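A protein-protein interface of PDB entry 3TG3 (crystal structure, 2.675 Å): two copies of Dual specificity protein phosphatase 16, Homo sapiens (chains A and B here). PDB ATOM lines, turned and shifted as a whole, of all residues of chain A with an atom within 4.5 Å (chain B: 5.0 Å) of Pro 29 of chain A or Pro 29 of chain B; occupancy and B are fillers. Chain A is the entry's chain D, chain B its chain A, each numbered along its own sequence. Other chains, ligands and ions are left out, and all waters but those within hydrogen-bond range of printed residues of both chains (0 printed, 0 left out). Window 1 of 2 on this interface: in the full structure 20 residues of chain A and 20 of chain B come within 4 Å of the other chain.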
ATOM      1  N   SER A  27      24.498  17.394 -25.013  1.00  0.00           N
ATOM      2  CA  SER A  27      23.950  16.184 -24.404  1.00  0.00           C
ATOM      3  C   SER A  27      23.250  16.457 -23.077  1.00  0.00           C
ATOM      4  O   SER A  27      22.562  15.585 -22.540  1.00  0.00           O
ATOM      5  CB  SER A  27      25.074  15.180 -24.152  1.00  0.00           C
ATOM      6  OG  SER A  27      26.059  15.713 -23.263  1.00  0.00           O
ATOM      7  N   ARG A  28      23.430  17.656 -22.534  1.00  0.00           N
ATOM      8  CA  ARG A  28      22.998  17.925 -21.159  1.00  0.00           C
ATOM      9  C   ARG A  28      21.481  17.933 -20.948  1.00  0.00           C
ATOM     10  O   ARG A  28      20.704  17.949 -21.902  1.00  0.00           O
ATOM     11  CB  ARG A  28      23.619  19.219 -20.631  1.00  0.00           C
ATOM     12  CG  ARG A  28      25.123  19.209 -20.569  1.00  0.00           C
ATOM     13  CD  ARG A  28      25.602  20.583 -20.224  1.00  0.00           C
ATOM     14  NE  ARG A  28      24.987  21.551 -21.122  1.00  0.00           N
ATOM     15  CZ  ARG A  28      24.864  22.846 -20.853  1.00  0.00           C
ATOM     16  NH1 ARG A  28      24.271  23.647 -21.729  1.00  0.00           N
ATOM     17  NH2 ARG A  28      25.321  23.342 -19.706  1.00  0.00           N
ATOM     18  N   PRO A  29      21.067  17.880 -19.673  1.00  0.00           N
ATOM     19  CA  PRO A  29      19.647  17.958 -19.342  1.00  0.00           C
ATOM     20  C   PRO A  29      19.020  19.207 -19.914  1.00  0.00           C
ATOM     21  O   PRO A  29      19.681  20.226 -20.085  1.00  0.00           O
ATOM     22  CB  PRO A  29      19.649  18.037 -17.828  1.00  0.00           C
ATOM     23  CG  PRO A  29      20.875  17.261 -17.446  1.00  0.00           C
ATOM     24  CD  PRO A  29      21.897  17.591 -18.488  1.00  0.00           C
ATOM     25  N   PHE A  30      17.728  19.102 -20.184  1.00  0.00           N
ATOM     26  CA  PHE A  30      16.956  20.163 -20.775  1.00  0.00           C
ATOM     27  C   PHE A  30      17.107  21.510 -20.056  1.00  0.00           C
ATOM     28  O   PHE A  30      17.254  22.547 -20.708  1.00  0.00           O
ATOM     29  CB  PHE A  30      15.494  19.751 -20.785  1.00  0.00           C
ATOM     30  CG  PHE A  30      14.601  20.761 -21.413  1.00  0.00           C
ATOM     31  CD1 PHE A  30      14.952  21.347 -22.620  1.00  0.00           C
ATOM     32  CD2 PHE A  30      13.411  21.126 -20.810  1.00  0.00           C
ATOM     33  CE1 PHE A  30      14.133  22.278 -23.211  1.00  0.00           C
ATOM     34  CE2 PHE A  30      12.587  22.059 -21.401  1.00  0.00           C
ATOM     35  CZ  PHE A  30      12.952  22.640 -22.602  1.00  0.00           C
ATOM     36  N   VAL A  31      17.042  21.498 -18.723  1.00  0.00           N
ATOM     37  CA  VAL A  31      17.179  22.723 -17.945  1.00  0.00           C
ATOM     38  C   VAL A  31      18.455  23.433 -18.318  1.00  0.00           C
ATOM     39  O   VAL A  31      18.465  24.625 -18.600  1.00  0.00           O
ATOM     40  CB  VAL A  31      17.298  22.436 -16.454  1.00  0.00           C
ATOM     41  CG1 VAL A  31      16.407  23.382 -15.666  1.00  0.00           C
ATOM     42  CG2 VAL A  31      16.935  21.003 -16.171  1.00  0.00           C
ATOM     43  N   GLU A  32      19.541  22.680 -18.285  1.00  0.00           N
ATOM     44  CA  GLU A  32      20.860  23.202 -18.554  1.00  0.00           C
ATOM     45  C   GLU A  32      20.943  23.791 -19.957  1.00  0.00           C
ATOM     46  O   GLU A  32      21.363  24.932 -20.147  1.00  0.00           O
ATOM     47  CB  GLU A  32      21.868  22.074 -18.400  1.00  0.00           C
ATOM     48  CG  GLU A  32      21.896  21.484 -17.016  1.00  0.00           C
ATOM     49  CD  GLU A  32      22.335  22.493 -15.972  1.00  0.00           C
ATOM     50  OE1 GLU A  32      23.549  22.562 -15.696  1.00  0.00           O
ATOM     51  OE2 GLU A  32      21.478  23.223 -15.434  1.00  0.00           O
ATOM     52  N   TYR A  33      20.561  23.002 -20.950  1.00  0.00           N
ATOM     53  CA  TYR A  33      20.544  23.495 -22.308  1.00  0.00           C
ATOM     54  C   TYR A  33      19.835  24.836 -22.365  1.00  0.00           C
ATOM     55  O   TYR A  33      20.300  25.774 -23.004  1.00  0.00           O
ATOM     56  CB  TYR A  33      19.829  22.519 -23.232  1.00  0.00           C
ATOM     57  CG  TYR A  33      19.827  23.011 -24.642  1.00  0.00           C
ATOM     58  CD1 TYR A  33      20.928  22.806 -25.464  1.00  0.00           C
ATOM     59  CD2 TYR A  33      18.752  23.718 -25.143  1.00  0.00           C
ATOM     60  CE1 TYR A  33      20.949  23.273 -26.762  1.00  0.00           C
ATOM     61  CE2 TYR A  33      18.744  24.186 -26.433  1.00  0.00           C
ATOM     62  CZ  TYR A  33      19.847  23.964 -27.247  1.00  0.00           C
ATOM     63  OH  TYR A  33      19.848  24.432 -28.547  1.00  0.00           O
ATOM     64  N   ASN A  45      18.866  15.869 -25.068  1.00  0.00           N
ATOM     65  CA  ASN A  45      19.007  16.055 -23.642  1.00  0.00           C
ATOM     66  C   ASN A  45      19.034  14.772 -22.865  1.00  0.00           C
ATOM     67  O   ASN A  45      18.286  13.841 -23.162  1.00  0.00           O
ATOM     68  CB  ASN A  45      17.906  16.960 -23.109  1.00  0.00           C
ATOM     69  CG  ASN A  45      16.535  16.515 -23.537  1.00  0.00           C
ATOM     70  OD1 ASN A  45      15.609  16.502 -22.741  1.00  0.00           O
ATOM     71  ND2 ASN A  45      16.396  16.146 -24.795  1.00  0.00           N
ATOM     72  N   CYS A  46      19.915  14.745 -21.867  1.00  0.00           N
ATOM     73  CA  CYS A  46      19.996  13.642 -20.926  1.00  0.00           C
ATOM     74  C   CYS A  46      18.660  13.507 -20.203  1.00  0.00           C
ATOM     75  O   CYS A  46      18.308  14.325 -19.346  1.00  0.00           O
ATOM     76  CB  CYS A  46      21.118  13.892 -19.938  1.00  0.00           C
ATOM     77  SG  CYS A  46      21.196  12.676 -18.682  1.00  0.00           S
ATOM     78  N   SER B  27      24.095  15.065  -7.458  1.00  0.00           N
ATOM     79  CA  SER B  27      23.428  16.199  -8.094  1.00  0.00           C
ATOM     80  C   SER B  27      22.878  15.863  -9.485  1.00  0.00           C
ATOM     81  O   SER B  27      22.127  16.643 -10.068  1.00  0.00           O
ATOM     82  CB  SER B  27      24.416  17.362  -8.211  1.00  0.00           C
ATOM     83  OG  SER B  27      25.529  17.003  -9.026  1.00  0.00           O
ATOM     84  N   ARG B  28      23.248  14.703 -10.010  1.00  0.00           N
ATOM     85  CA  ARG B  28      22.999  14.398 -11.427  1.00  0.00           C
ATOM     86  C   ARG B  28      21.527  14.166 -11.788  1.00  0.00           C
ATOM     87  O   ARG B  28      20.684  13.950 -10.922  1.00  0.00           O
ATOM     88  CB  ARG B  28      23.850  13.214 -11.891  1.00  0.00           C
ATOM     89  CG  ARG B  28      25.358  13.449 -11.796  1.00  0.00           C
ATOM     90  CD  ARG B  28      26.083  12.162 -12.079  1.00  0.00           C
ATOM     91  NE  ARG B  28      25.462  11.083 -11.311  1.00  0.00           N
ATOM     92  CZ  ARG B  28      25.557   9.788 -11.599  1.00  0.00           C
ATOM     93  NH1 ARG B  28      24.955   8.906 -10.817  1.00  0.00           N
ATOM     94  NH2 ARG B  28      26.250   9.371 -12.656  1.00  0.00           N
ATOM     95  N   PRO B  29      21.219  14.230 -13.087  1.00  0.00           N
ATOM     96  CA  PRO B  29      19.859  13.959 -13.536  1.00  0.00           C
ATOM     97  C   PRO B  29      19.383  12.628 -13.005  1.00  0.00           C
ATOM     98  O   PRO B  29      20.182  11.738 -12.688  1.00  0.00           O
ATOM     99  CB  PRO B  29      20.000  13.900 -15.065  1.00  0.00           C
ATOM    100  CG  PRO B  29      21.162  14.798 -15.356  1.00  0.00           C
ATOM    101  CD  PRO B  29      22.113  14.593 -14.208  1.00  0.00           C
ATOM    102  N   PHE B  30      18.064  12.510 -12.930  1.00  0.00           N
ATOM    103  CA  PHE B  30      17.400  11.350 -12.373  1.00  0.00           C
ATOM    104  C   PHE B  30      17.793  10.049 -13.068  1.00  0.00           C
ATOM    105  O   PHE B  30      18.042   9.044 -12.416  1.00  0.00           O
ATOM    106  CB  PHE B  30      15.895  11.560 -12.466  1.00  0.00           C
ATOM    107  CG  PHE B  30      15.103  10.429 -11.932  1.00  0.00           C
ATOM    108  CD1 PHE B  30      15.429   9.869 -10.711  1.00  0.00           C
ATOM    109  CD2 PHE B  30      14.027   9.925 -12.641  1.00  0.00           C
ATOM    110  CE1 PHE B  30      14.697   8.829 -10.198  1.00  0.00           C
ATOM    111  CE2 PHE B  30      13.290   8.879 -12.138  1.00  0.00           C
ATOM    112  CZ  PHE B  30      13.624   8.328 -10.911  1.00  0.00           C
ATOM    113  N   VAL B  31      17.831  10.069 -14.394  1.00  0.00           N
ATOM    114  CA  VAL B  31      18.203   8.884 -15.162  1.00  0.00           C
ATOM    115  C   VAL B  31      19.552   8.376 -14.682  1.00  0.00           C
ATOM    116  O   VAL B  31      19.707   7.189 -14.392  1.00  0.00           O
ATOM    117  CB  VAL B  31      18.368   9.170 -16.683  1.00  0.00           C
ATOM    118  CG1 VAL B  31      17.618   8.147 -17.474  1.00  0.00           C
ATOM    119  CG2 VAL B  31      17.901  10.547 -17.032  1.00  0.00           C
ATOM    120  N   GLU B  32      20.530   9.279 -14.621  1.00  0.00           N
ATOM    121  CA  GLU B  32      21.889   8.919 -14.257  1.00  0.00           C
ATOM    122  C   GLU B  32      21.926   8.319 -12.859  1.00  0.00           C
ATOM    123  O   GLU B  32      22.472   7.242 -12.645  1.00  0.00           O
ATOM    124  CB  GLU B  32      22.785  10.151 -14.312  1.00  0.00           C
ATOM    125  CG  GLU B  32      22.819  10.808 -15.653  1.00  0.00           C
ATOM    126  CD  GLU B  32      23.434   9.907 -16.692  1.00  0.00           C
ATOM    127  OE1 GLU B  32      24.647  10.061 -16.951  1.00  0.00           O
ATOM    128  OE2 GLU B  32      22.716   9.029 -17.224  1.00  0.00           O
ATOM    129  N   TYR B  33      21.352   9.030 -11.903  1.00  0.00           N
ATOM    130  CA  TYR B  33      21.293   8.505 -10.550  1.00  0.00           C
ATOM    131  C   TYR B  33      20.754   7.080 -10.540  1.00  0.00           C
ATOM    132  O   TYR B  33      21.257   6.205  -9.837  1.00  0.00           O
ATOM    133  CB  TYR B  33      20.388   9.364  -9.677  1.00  0.00           C
ATOM    134  CG  TYR B  33      20.330   8.835  -8.280  1.00  0.00           C
ATOM    135  CD1 TYR B  33      21.330   9.140  -7.367  1.00  0.00           C
ATOM    136  CD2 TYR B  33      19.287   8.006  -7.874  1.00  0.00           C
ATOM    137  CE1 TYR B  33      21.287   8.660  -6.081  1.00  0.00           C
ATOM    138  CE2 TYR B  33      19.235   7.520  -6.575  1.00  0.00           C
ATOM    139  CZ  TYR B  33      20.239   7.848  -5.694  1.00  0.00           C
ATOM    140  OH  TYR B  33      20.185   7.360  -4.418  1.00  0.00           O
ATOM    141  N   ASN B  43      19.740  11.631  -4.125  1.00  0.00           N
ATOM    142  CA  ASN B  43      19.550  12.272  -5.420  1.00  0.00           C
ATOM    143  C   ASN B  43      18.799  13.599  -5.313  1.00  0.00           C
ATOM    144  O   ASN B  43      17.573  13.627  -5.176  1.00  0.00           O
ATOM    145  CB  ASN B  43      18.828  11.328  -6.380  1.00  0.00           C
ATOM    146  CG  ASN B  43      18.970  11.745  -7.837  1.00  0.00           C
ATOM    147  OD1 ASN B  43      18.271  11.226  -8.719  1.00  0.00           O
ATOM    148  ND2 ASN B  43      19.886  12.672  -8.096  1.00  0.00           N
ATOM    149  N   ASN B  45      18.380  15.726  -7.908  1.00  0.00           N
ATOM    150  CA  ASN B  45      18.626  15.626  -9.335  1.00  0.00           C
ATOM    151  C   ASN B  45      18.505  16.919 -10.107  1.00  0.00           C
ATOM    152  O   ASN B  45      17.600  17.725  -9.875  1.00  0.00           O
ATOM    153  CB  ASN B  45      17.701  14.582  -9.957  1.00  0.00           C
ATOM    154  CG  ASN B  45      16.255  14.819  -9.626  1.00  0.00           C
ATOM    155  OD1 ASN B  45      15.401  14.755 -10.493  1.00  0.00           O
ATOM    156  ND2 ASN B  45      15.966  15.074  -8.352  1.00  0.00           N
ATOM    157  N   CYS B  46      19.436  17.088 -11.044  1.00  0.00           N
ATOM    158  CA  CYS B  46      19.457  18.225 -11.945  1.00  0.00           C
ATOM    159  C   CYS B  46      18.192  18.193 -12.772  1.00  0.00           C
ATOM    160  O   CYS B  46      18.030  17.373 -13.673  1.00  0.00           O
ATOM    161  CB  CYS B  46      20.691  18.166 -12.838  1.00  0.00           C
ATOM    162  SG  CYS B  46      20.705  19.365 -14.186  1.00  0.00           S
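Pro 29 of chain B touches Pro 29 of chain A (CG to CG, 3.2 Å).
Pro 29 of chain A touches Cys 46 of chain B (CG to SG, 3.9 Å).
Glu 32 of chain A touches Cys 46 of chain B.
Pro 29 of chain B touches Cys 46 of chain A (CG to SG, 3.9 Å).
Cys 46 of chain A touches Glu 32 of chain B (SG to CG, 3.9 Å).
O of Arg 28 of chain A lies within hydrogen-bond range of N of Cys 46 of chain A (3.3 Å).
The backbone carbonyl oxygen (O) of Arg 28 of chain B is in hydrogen-bond range of the backbone NH (N) of Cys 46 of chain B (3.4 Å).
The backbone carbonyl oxygen of Ser 27 of chain B is in hydrogen-bond range of the backbone NH of Cys 46 of chain B, 2.9 Å away.
N of Cys 46 of chain A is in hydrogen-bond range of O of Ser 27 of chain A, 2.9 Å away.
Pro 29 of chain A touches its own counterpart, Pro 29 of chain B.
Pro 29 of chain A touches Cys 46 of chain B, and with the chains exchanged Cys 46 of chain A touches Pro 29 of chain B.
Glu 32 of chain A touches Cys 46 of chain B, and with the chains exchanged Cys 46 of chain A touches Glu 32 of chain B.
Positions printed for both chains: 27, 28, 29, 30, 31, 32, 33, 45 and 46.
Of the 5 pairs that touch across the chains among the printed residues, 5 have their exchanged pair printed and touching as well.
Arg 28 of chain A touches none of the printed residues of chain B.
Of the printed residues of chain B, Pro 29 of chain A touches Pro 29 (3.2 Å) and Cys 46 (3.9 Å).
Printed residues of chain B within 4 Å of Glu 32 of chain A: Cys 46.
Printed residues of chain B within 4 Å of Cys 46 of chain A: Pro 29 and Glu 32.
Of chain A, only Pro 29 (3.2 Å) and Cys 46 (3.9 Å) come within 4 Å of Pro 29 of chain B.
Of the printed residues of chain A, Glu 32 of chain B touches Cys 46.
Printed residues of chain A within 4 Å of Cys 46 of chain B: Pro 29 (3.9 Å) and Glu 32 (3.7 Å).
The nearest printed residue of chain A that does not touch Pro 29 of chain B is Arg 28 of chain A (6.4 Å).
The nearest printed residue of chain B that does not touch Glu 32 of chain A is Pro 29 of chain B (6.9 Å).
Hydrophobic or aromatic side chains of chain B that line the printed part of chain A: Pro 29.
Of the 9 printed residues of chain A, 3 touch a printed residue of chain B.
Among the printed residues, 5 pairs touch across the chains.
Among the printed residues, no Asp or Glu carboxylate lies within 4 Å of a Lys or Arg side-chain nitrogen of the other chain.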
